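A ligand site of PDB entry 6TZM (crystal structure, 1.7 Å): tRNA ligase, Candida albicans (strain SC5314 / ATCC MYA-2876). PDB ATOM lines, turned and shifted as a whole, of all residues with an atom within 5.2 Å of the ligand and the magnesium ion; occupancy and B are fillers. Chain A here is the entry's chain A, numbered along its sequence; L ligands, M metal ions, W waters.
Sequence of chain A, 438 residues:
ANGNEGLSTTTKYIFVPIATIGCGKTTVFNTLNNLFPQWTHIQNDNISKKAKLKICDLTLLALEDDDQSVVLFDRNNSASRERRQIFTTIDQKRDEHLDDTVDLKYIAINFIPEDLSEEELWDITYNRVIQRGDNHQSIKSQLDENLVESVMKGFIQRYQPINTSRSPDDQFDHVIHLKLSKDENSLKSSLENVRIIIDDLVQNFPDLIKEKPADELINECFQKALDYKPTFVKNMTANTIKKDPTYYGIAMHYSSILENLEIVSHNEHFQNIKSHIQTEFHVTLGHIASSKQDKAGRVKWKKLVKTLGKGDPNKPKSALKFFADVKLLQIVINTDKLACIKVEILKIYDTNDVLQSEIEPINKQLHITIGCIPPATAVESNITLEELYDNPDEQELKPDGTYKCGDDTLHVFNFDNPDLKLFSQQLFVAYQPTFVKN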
ATOM      1  N   THR A  20      -4.751  10.036  16.345  1.00  0.00           N
ATOM      2  CA  THR A  20      -3.957   9.115  15.534  1.00  0.00           C
ATOM      3  C   THR A  20      -4.656   7.758  15.538  1.00  0.00           C
ATOM      4  O   THR A  20      -5.712   7.588  16.153  1.00  0.00           O
ATOM      5  CB  THR A  20      -2.520   9.033  16.040  1.00  0.00           C
ATOM      6  OG1 THR A  20      -2.509   8.621  17.412  1.00  0.00           O
ATOM      7  CG2 THR A  20      -1.819  10.390  15.906  1.00  0.00           C
ATOM      8  N   ILE A  21      -4.061   6.774  14.849  1.00  0.00           N
ATOM      9  CA  ILE A  21      -4.690   5.454  14.729  1.00  0.00           C
ATOM     10  C   ILE A  21      -4.784   4.790  16.090  1.00  0.00           C
ATOM     11  O   ILE A  21      -3.805   4.743  16.847  1.00  0.00           O
ATOM     12  CB  ILE A  21      -3.904   4.571  13.750  1.00  0.00           C
ATOM     13  CG1 ILE A  21      -3.974   5.168  12.334  1.00  0.00           C
ATOM     14  CG2 ILE A  21      -4.454   3.161  13.778  1.00  0.00           C
ATOM     15  CD1 ILE A  21      -3.249   4.348  11.307  1.00  0.00           C
ATOM     16  N   GLY A  22      -5.955   4.236  16.402  1.00  0.00           N
ATOM     17  CA  GLY A  22      -6.127   3.443  17.607  1.00  0.00           C
ATOM     18  C   GLY A  22      -6.474   4.237  18.847  1.00  0.00           C
ATOM     19  O   GLY A  22      -6.523   3.667  19.935  1.00  0.00           O
ATOM     20  N   CYS A  23      -6.703   5.547  18.710  1.00  0.00           N
ATOM     21  CA  CYS A  23      -7.115   6.342  19.868  1.00  0.00           C
ATOM     22  C   CYS A  23      -8.538   6.069  20.314  1.00  0.00           C
ATOM     23  O   CYS A  23      -8.921   6.544  21.384  1.00  0.00           O
ATOM     24  CB  CYS A  23      -6.983   7.842  19.592  1.00  0.00           C
ATOM     25  SG  CYS A  23      -5.264   8.498  19.461  1.00  0.00           S
ATOM     26  N   GLY A  24      -9.303   5.311  19.537  1.00  0.00           N
ATOM     27  CA  GLY A  24     -10.673   4.997  19.863  1.00  0.00           C
ATOM     28  C   GLY A  24     -11.727   5.819  19.145  1.00  0.00           C
ATOM     29  O   GLY A  24     -12.883   5.832  19.592  1.00  0.00           O
ATOM     30  N   LYS A  25     -11.366   6.493  18.032  1.00  0.00           N
ATOM     31  CA  LYS A  25     -12.349   7.311  17.317  1.00  0.00           C
ATOM     32  C   LYS A  25     -13.571   6.502  16.917  1.00  0.00           C
ATOM     33  O   LYS A  25     -14.704   6.909  17.175  1.00  0.00           O
ATOM     34  CB  LYS A  25     -11.746   7.918  16.038  1.00  0.00           C
ATOM     35  CG  LYS A  25     -10.513   8.731  16.219  1.00  0.00           C
ATOM     36  CD  LYS A  25     -10.069   9.267  14.840  1.00  0.00           C
ATOM     37  CE  LYS A  25      -9.668   8.133  13.911  1.00  0.00           C
ATOM     38  NZ  LYS A  25      -8.447   7.413  14.414  1.00  0.00           N
ATOM     39  N   THR A  26     -13.345   5.385  16.221  1.00  0.00           N
ATOM     40  CA  THR A  26     -14.483   4.621  15.712  1.00  0.00           C
ATOM     41  C   THR A  26     -15.303   4.035  16.853  1.00  0.00           C
ATOM     42  O   THR A  26     -16.530   3.988  16.776  1.00  0.00           O
ATOM     43  CB  THR A  26     -13.984   3.534  14.767  1.00  0.00           C
ATOM     44  OG1 THR A  26     -13.273   4.162  13.683  1.00  0.00           O
ATOM     45  CG2 THR A  26     -15.143   2.715  14.200  1.00  0.00           C
ATOM     46  N   THR A  27     -14.630   3.619  17.935  1.00  0.00           N
ATOM     47  CA  THR A  27     -15.348   3.051  19.068  1.00  0.00           C
ATOM     48  C   THR A  27     -16.224   4.104  19.733  1.00  0.00           C
ATOM     49  O   THR A  27     -17.404   3.848  20.028  1.00  0.00           O
ATOM     50  CB  THR A  27     -14.354   2.445  20.067  1.00  0.00           C
ATOM     51  OG1 THR A  27     -13.580   1.438  19.401  1.00  0.00           O
ATOM     52  CG2 THR A  27     -15.091   1.831  21.259  1.00  0.00           C
ATOM     53  N   VAL A  28     -15.666   5.296  19.942  1.00  0.00           N
ATOM     54  CA  VAL A  28     -16.409   6.399  20.566  1.00  0.00           C
ATOM     55  C   VAL A  28     -17.584   6.801  19.675  1.00  0.00           C
ATOM     56  O   VAL A  28     -18.723   6.963  20.131  1.00  0.00           O
ATOM     57  CB  VAL A  28     -15.467   7.580  20.835  1.00  0.00           C
ATOM     58  CG1 VAL A  28     -16.261   8.830  21.183  1.00  0.00           C
ATOM     59  CG2 VAL A  28     -14.523   7.226  21.993  1.00  0.00           C
ATOM     60  N   ASP A  45     -12.332   5.597   6.514  1.00  0.00           N
ATOM     61  CA  ASP A  45     -11.760   4.296   6.178  1.00  0.00           C
ATOM     62  C   ASP A  45     -12.666   3.468   5.271  1.00  0.00           C
ATOM     63  O   ASP A  45     -12.180   2.565   4.586  1.00  0.00           O
ATOM     64  CB  ASP A  45     -11.452   3.509   7.459  1.00  0.00           C
ATOM     65  CG  ASP A  45      -9.992   3.575   7.853  1.00  0.00           C
ATOM     66  OD1 ASP A  45      -9.144   3.124   7.050  1.00  0.00           O
ATOM     67  OD2 ASP A  45      -9.696   4.080   8.962  1.00  0.00           O
ATOM     68  N   ASP A  74     -15.383  10.866  10.910  1.00  0.00           N
ATOM     69  CA  ASP A  74     -14.443   9.872  11.452  1.00  0.00           C
ATOM     70  C   ASP A  74     -13.196   9.786  10.577  1.00  0.00           C
ATOM     71  O   ASP A  74     -13.123   9.003   9.621  1.00  0.00           O
ATOM     72  CB  ASP A  74     -15.145   8.529  11.587  1.00  0.00           C
ATOM     73  CG  ASP A  74     -14.363   7.528  12.419  1.00  0.00           C
ATOM     74  OD1 ASP A  74     -13.145   7.708  12.646  1.00  0.00           O
ATOM     75  OD2 ASP A  74     -14.987   6.539  12.871  1.00  0.00           O
ATOM     76  N   ASN A  76      -8.637  10.886  11.192  1.00  0.00           N
ATOM     77  CA  ASN A  76      -7.658  11.242  12.214  1.00  0.00           C
ATOM     78  C   ASN A  76      -7.486  12.751  12.343  1.00  0.00           C
ATOM     79  O   ASN A  76      -7.526  13.285  13.459  1.00  0.00           O
ATOM     80  CB  ASN A  76      -6.317  10.583  11.926  1.00  0.00           C
ATOM     81  CG  ASN A  76      -6.276   9.156  12.394  1.00  0.00           C
ATOM     82  OD1 ASN A  76      -6.523   8.887  13.563  1.00  0.00           O
ATOM     83  ND2 ASN A  76      -6.019   8.235  11.499  1.00  0.00           N
ATOM     84  N   ARG A 128      -3.248  -1.474  21.541  1.00  0.00           N
ATOM     85  CA  ARG A 128      -4.638  -1.630  21.137  1.00  0.00           C
ATOM     86  C   ARG A 128      -4.745  -2.232  19.743  1.00  0.00           C
ATOM     87  O   ARG A 128      -5.556  -3.141  19.496  1.00  0.00           O
ATOM     88  CB  ARG A 128      -5.349  -0.275  21.175  1.00  0.00           C
ATOM     89  CG  ARG A 128      -5.767   0.181  22.571  1.00  0.00           C
ATOM     90  CD  ARG A 128      -6.508   1.508  22.436  1.00  0.00           C
ATOM     91  NE  ARG A 128      -6.804   2.152  23.725  1.00  0.00           N
ATOM     92  CZ  ARG A 128      -7.307   3.376  23.825  1.00  0.00           C
ATOM     93  NH1 ARG A 128      -7.584   4.069  22.723  1.00  0.00           N
ATOM     94  NH2 ARG A 128      -7.560   3.913  25.017  1.00  0.00           N
ATOM     95  N   VAL A 129      -3.925  -1.757  18.814  1.00  0.00           N
ATOM     96  CA  VAL A 129      -4.111  -2.121  17.408  1.00  0.00           C
ATOM     97  C   VAL A 129      -3.586  -3.526  17.130  1.00  0.00           C
ATOM     98  O   VAL A 129      -4.222  -4.297  16.407  1.00  0.00           O
ATOM     99  CB  VAL A 129      -3.469  -1.058  16.498  1.00  0.00           C
ATOM    100  CG1 VAL A 129      -3.436  -1.540  15.052  1.00  0.00           C
ATOM    101  CG2 VAL A 129      -4.218   0.262  16.625  1.00  0.00           C
ATOM    102  N   GLN A 131      -3.510  -5.878  19.297  1.00  0.00           N
ATOM    103  CA  GLN A 131      -4.410  -6.757  20.048  1.00  0.00           C
ATOM    104  C   GLN A 131      -5.834  -6.681  19.516  1.00  0.00           C
ATOM    105  O   GLN A 131      -6.070  -6.379  18.349  1.00  0.00           O
ATOM    106  CB  GLN A 131      -4.383  -6.410  21.529  1.00  0.00           C
ATOM    107  CG  GLN A 131      -5.198  -7.350  22.406  1.00  0.00           C
ATOM    108  CD  GLN A 131      -5.101  -7.007  23.891  1.00  0.00           C
ATOM    109  OE1 GLN A 131      -4.716  -5.901  24.264  1.00  0.00           O
ATOM    110  NE2 GLN A 131      -5.435  -7.971  24.744  1.00  0.00           N
ATOM    111  N   ASP A 183      -6.367   1.577  30.705  1.00  0.00           N
ATOM    112  CA  ASP A 183      -7.607   1.367  31.425  1.00  0.00           C
ATOM    113  C   ASP A 183      -7.278   1.145  32.892  1.00  0.00           C
ATOM    114  O   ASP A 183      -6.328   0.431  33.235  1.00  0.00           O
ATOM    115  CB  ASP A 183      -8.375   0.181  30.827  1.00  0.00           C
ATOM    116  CG  ASP A 183      -8.558   0.305  29.308  1.00  0.00           C
ATOM    117  OD1 ASP A 183      -8.924   1.401  28.840  1.00  0.00           O
ATOM    118  OD2 ASP A 183      -8.305  -0.668  28.585  1.00  0.00           O
ATOM    119  N   LYS A 188     -12.898   1.304  30.671  1.00  0.00           N
ATOM    120  CA  LYS A 188     -12.222   1.600  29.416  1.00  0.00           C
ATOM    121  C   LYS A 188     -12.141   3.109  29.204  1.00  0.00           C
ATOM    122  O   LYS A 188     -13.093   3.848  29.466  1.00  0.00           O
ATOM    123  CB  LYS A 188     -12.956   0.963  28.242  1.00  0.00           C
ATOM    124  CG  LYS A 188     -13.069  -0.547  28.315  1.00  0.00           C
ATOM    125  CD  LYS A 188     -11.880  -1.238  27.721  1.00  0.00           C
ATOM    126  CE  LYS A 188     -12.083  -2.748  27.723  1.00  0.00           C
ATOM    127  NZ  LYS A 188     -12.097  -3.283  29.111  1.00  0.00           N
ATOM    128  N   SER A 189     -10.981   3.546  28.697  1.00  0.00           N
ATOM    129  CA  SER A 189     -10.759   4.957  28.424  1.00  0.00           C
ATOM    130  C   SER A 189     -11.828   5.514  27.497  1.00  0.00           C
ATOM    131  O   SER A 189     -12.389   6.592  27.755  1.00  0.00           O
ATOM    132  CB  SER A 189      -9.352   5.117  27.829  1.00  0.00           C
ATOM    133  OG  SER A 189      -9.078   6.467  27.543  1.00  0.00           O
ATOM    134  N   SER A 190     -12.159   4.772  26.436  1.00  0.00           N
ATOM    135  CA  SER A 190     -13.167   5.254  25.481  1.00  0.00           C
ATOM    136  C   SER A 190     -14.560   5.362  26.114  1.00  0.00           C
ATOM    137  O   SER A 190     -15.351   6.214  25.690  1.00  0.00           O
ATOM    138  CB  SER A 190     -13.228   4.339  24.251  1.00  0.00           C
ATOM    139  OG  SER A 190     -12.005   4.372  23.520  1.00  0.00           O
ATOM    140  N   LEU A 191     -14.883   4.520  27.086  1.00  0.00           N
ATOM    141  CA  LEU A 191     -16.192   4.644  27.740  1.00  0.00           C
ATOM    142  C   LEU A 191     -16.240   5.900  28.596  1.00  0.00           C
ATOM    143  O   LEU A 191     -17.227   6.638  28.581  1.00  0.00           O
ATOM    144  CB  LEU A 191     -16.503   3.398  28.573  1.00  0.00           C
ATOM    145  CG  LEU A 191     -17.772   3.484  29.435  1.00  0.00           C
ATOM    146  CD1 LEU A 191     -18.986   3.693  28.553  1.00  0.00           C
ATOM    147  CD2 LEU A 191     -17.957   2.240  30.315  1.00  0.00           C
ATOM    148  N   PHE A 222     -21.821   1.106  24.537  1.00  0.00           N
ATOM    149  CA  PHE A 222     -20.366   0.994  24.419  1.00  0.00           C
ATOM    150  C   PHE A 222     -19.944  -0.463  24.257  1.00  0.00           C
ATOM    151  O   PHE A 222     -19.080  -0.764  23.421  1.00  0.00           O
ATOM    152  CB  PHE A 222     -19.696   1.619  25.640  1.00  0.00           C
ATOM    153  CG  PHE A 222     -18.219   1.437  25.662  1.00  0.00           C
ATOM    154  CD1 PHE A 222     -17.406   2.244  24.878  1.00  0.00           C
ATOM    155  CD2 PHE A 222     -17.624   0.459  26.452  1.00  0.00           C
ATOM    156  CE1 PHE A 222     -16.031   2.088  24.877  1.00  0.00           C
ATOM    157  CE2 PHE A 222     -16.250   0.303  26.451  1.00  0.00           C
ATOM    158  CZ  PHE A 222     -15.459   1.117  25.666  1.00  0.00           C
ATOM    159  N   LEU A 226     -17.536  -1.741  21.506  1.00  0.00           N
ATOM    160  CA  LEU A 226     -16.251  -2.318  21.903  1.00  0.00           C
ATOM    161  C   LEU A 226     -16.061  -3.697  21.308  1.00  0.00           C
ATOM    162  O   LEU A 226     -15.017  -3.997  20.712  1.00  0.00           O
ATOM    163  CB  LEU A 226     -16.154  -2.367  23.427  1.00  0.00           C
ATOM    164  CG  LEU A 226     -14.821  -2.905  23.913  1.00  0.00           C
ATOM    165  CD1 LEU A 226     -13.758  -1.866  23.610  1.00  0.00           C
ATOM    166  CD2 LEU A 226     -14.903  -3.206  25.392  1.00  0.00           C
ATOM    167  N   LYS A 229     -16.494  -6.697  15.862  1.00  0.00           N
ATOM    168  CA  LYS A 229     -15.399  -7.277  15.105  1.00  0.00           C
ATOM    169  C   LYS A 229     -15.659  -7.150  13.607  1.00  0.00           C
ATOM    170  O   LYS A 229     -16.424  -7.940  13.033  1.00  0.00           O
ATOM    171  CB  LYS A 229     -15.197  -8.743  15.496  1.00  0.00           C
ATOM    172  CG  LYS A 229     -14.951  -8.969  16.985  1.00  0.00           C
ATOM    173  CD  LYS A 229     -13.775  -8.139  17.502  1.00  0.00           C
ATOM    174  CE  LYS A 229     -14.128  -7.450  18.827  1.00  0.00           C
ATOM    175  NZ  LYS A 229     -13.478  -6.124  18.981  1.00  0.00           N
HETATM  176  P1  LIG L   1      -9.482   4.214  15.789  1.00  0.00           P
HETATM  177  O1  LIG L   1     -10.803   4.274  15.095  1.00  0.00           O
HETATM  178  O2  LIG L   1      -9.139   5.577  16.361  1.00  0.00           O
HETATM  179  O3  LIG L   1      -8.365   3.777  14.899  1.00  0.00           O
HETATM  180  O4  LIG L   1      -9.550   3.242  17.096  1.00  0.00           O
HETATM  181  P2  LIG L   1     -10.655   2.133  17.360  1.00  0.00           P
HETATM  182  O5  LIG L   1     -11.950   2.704  17.884  1.00  0.00           O
HETATM  183  O6  LIG L   1     -10.851   1.255  16.142  1.00  0.00           O
HETATM  184  O7  LIG L   1      -9.984   1.279  18.545  1.00  0.00           O
HETATM  185  C1  LIG L   1      -8.813   0.515  18.236  1.00  0.00           C
HETATM  186  C2  LIG L   1      -8.823  -0.781  19.032  1.00  0.00           C
HETATM  187  O8  LIG L   1      -8.796  -0.464  20.415  1.00  0.00           O
HETATM  188  C3  LIG L   1     -10.102  -1.573  18.795  1.00  0.00           C
HETATM  189  O9  LIG L   1      -9.738  -2.964  18.821  1.00  0.00           O
HETATM  190  C4  LIG L   1     -10.984  -1.206  19.976  1.00  0.00           C
HETATM  191  O10 LIG L   1     -11.914  -2.230  20.345  1.00  0.00           O
HETATM  192  C5  LIG L   1      -9.961  -0.959  21.072  1.00  0.00           C
HETATM  193  N1  LIG L   1     -10.323   0.089  22.047  1.00  0.00           N
HETATM  194  C6  LIG L   1     -10.988   1.260  21.833  1.00  0.00           C
HETATM  195  N2  LIG L   1     -11.076   1.982  22.986  1.00  0.00           N
HETATM  196  C7  LIG L   1     -10.444   1.267  23.944  1.00  0.00           C
HETATM  197  C8  LIG L   1     -10.165   1.427  25.381  1.00  0.00           C
HETATM  198  O11 LIG L   1     -10.533   2.443  26.012  1.00  0.00           O
HETATM  199  N3  LIG L   1      -9.471   0.442  25.980  1.00  0.00           N
HETATM  200  C9  LIG L   1      -9.045  -0.664  25.344  1.00  0.00           C
HETATM  201  N4  LIG L   1      -8.361  -1.605  26.056  1.00  0.00           N
HETATM  202  N5  LIG L   1      -9.257  -0.885  24.028  1.00  0.00           N
HETATM  203  C10 LIG L   1      -9.944   0.043  23.306  1.00  0.00           C
HETATM  204 MG    MG M   1     -11.336   3.783  13.057  1.00  0.00          MG
HETATM  205  O   HOH W   1     -11.425  -4.809  18.407  1.00  0.00           O
HETATM  206  O   HOH W   2      -6.795  -3.826  25.024  1.00  0.00           O
HETATM  207  O   HOH W   3      -7.732   5.714  12.461  1.00  0.00           O
HETATM  208  O   HOH W   4      -7.815  -3.846  20.837  1.00  0.00           O
HETATM  209  O   HOH W   5     -11.319   5.886  12.279  1.00  0.00           O
HETATM  210  O   HOH W   6      -5.754   0.563  25.938  1.00  0.00           O
HETATM  211  O   HOH W   7     -13.415   0.074  16.260  1.00  0.00           O
HETATM  212  O   HOH W   8     -11.473   1.636  13.494  1.00  0.00           O
HETATM  213  O   HOH W   9     -11.801  -4.728  21.563  1.00  0.00           O
HETATM  214  O   HOH W  10     -14.088  -1.276  18.930  1.00  0.00           O
HETATM  215  O   HOH W  11      -9.352   3.443  12.382  1.00  0.00           O
HETATM  216  O   HOH W  12     -11.869   3.265  10.975  1.00  0.00           O
HETATM  217  O   HOH W  13      -8.089  -2.725  15.972  1.00  0.00           O
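The guanidinium group of Arg 128 is in hydrogen-bond range of the backbone carbonyl oxygen of Cys 23 (3.1 Å). N of Ile 21 sits at hydrogen-bond distance from OD1 of Asn 76, 3.5 Å away. The side-chain amino group (NZ) of Lys 25 is in hydrogen-bond range of the side-chain amide oxygen (OD1) of Asn 76 (2.6 Å). O of Thr 20 lies within hydrogen-bond range of NZ of Lys 25 (3.2 Å). The side-chain hydroxyl (OG1) of Thr 20 is in hydrogen-bond range of the side-chain sulfur (SG) of Cys 23 (3.4 Å). OD2 of Asp 74 lies close to OG1 of Thr 26 (3.0 Å). O of Leu 226 sits at hydrogen-bond distance from NZ of Lys 229 (3.1 Å). The side-chain carboxylate (OD1) of Asp 183 sits at hydrogen-bond distance from the backbone NH (N) of Ser 189 (3.0 Å).
Of the 23 residues printed, 1 comes within 4 Å of the magnesium ion. The nearest printed residue that does not touch the magnesium ion is Asp 74 (4.3 Å).
Water W11 bridges an oxygen (O3) of the ligand (2.7 Å) and the side-chain carboxylate (OD2) of Asp 45 (3.5 Å). Water W1 lies within hydrogen-bond range of the side-chain amino group of Lys 229 (2.5 Å) and an oxygen (O9) of the ligand (2.5 Å). Water W10 lies within hydrogen-bond range of an oxygen (O10) of the ligand (2.8 Å), the side-chain hydroxyl (OG1) of Thr 27 (2.8 Å) and the backbone carbonyl oxygen (O) of Leu 226 (3.4 Å). Water W7 lies within hydrogen-bond range of O6 of the ligand (2.8 Å) and OG1 of Thr 27 (3.4 Å). Water W2 bridges a nitrogen (N4) of the ligand (2.9 Å) and the side-chain amide oxygen of Gln 131 (3.0 Å). Water W3 lies within hydrogen-bond range of the side-chain amino group (NZ) of Lys 25 (2.7 Å), an oxygen (O3) of the ligand (3.2 Å) and the side-chain amide nitrogen (ND2) of Asn 76 (3.2 Å).
Merely in contact with the ligand: Lys 188, Leu 226, Ile 21 and Thr 20. 14 residues have an atom within 4 Å of the ligand: Thr 20, Ile 21, Gly 22, Cys 23, Gly 24, Lys 25, Thr 26, Thr 27, Arg 128, Asp 183, Lys 188, Ser 189, Ser 190 and Leu 226.
N of Thr 26 lies within hydrogen-bond range of O5 of the ligand (3.4 Å). The guanidinium group (NH2) of Arg 128 is in hydrogen-bond range of an oxygen (O11) of the ligand (3.5 Å). An oxygen (O2) of the ligand is in hydrogen-bond range of the backbone NH (N) of Lys 25 (2.9 Å). The backbone NH (N) of Thr 27 lies within hydrogen-bond range of an oxygen (O5) of the ligand (2.8 Å). The backbone NH (N) of Gly 24 sits at hydrogen-bond distance from an oxygen (O2) of the ligand. A nitrogen (N2) of the ligand sits at hydrogen-bond distance from the side-chain hydroxyl (OG) of Ser 190 (2.6 Å). N of Ser 190 sits at hydrogen-bond distance from O11 of the ligand, 2.9 Å away. A nitrogen (N4) of the ligand is in hydrogen-bond range of the side-chain carboxylate (OD2) of Asp 183. The side-chain hydroxyl (OG1) of Thr 27 is in hydrogen-bond range of an oxygen (O5) of the ligand, 2.6 Å away. An oxygen (O11) of the ligand lies within hydrogen-bond range of the backbone NH of Ser 189 (2.9 Å). The backbone NH (N) of Gly 22 sits at hydrogen-bond distance from an oxygen (O3) of the ligand, at 2.9 Å. The backbone NH (N) of Cys 23 lies within hydrogen-bond range of an oxygen (O2) of the ligand, at 3.4 Å. O2 of the ligand is in salt-bridge range of NZ of Lys 25, at 2.8 Å.
The side-chain hydroxyl (OG1) of Thr 26 binds the magnesium ion, 2.1 Å away. The magnesium ion is bound by water W11, at 2.1 Å. O1 of the ligand is bound to the magnesium ion (2.2 Å). Water W8 binds the magnesium ion (2.2 Å). The magnesium ion is bound by water W12 (2.2 Å). Water W5 is bound to the magnesium ion, at 2.2 Å.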
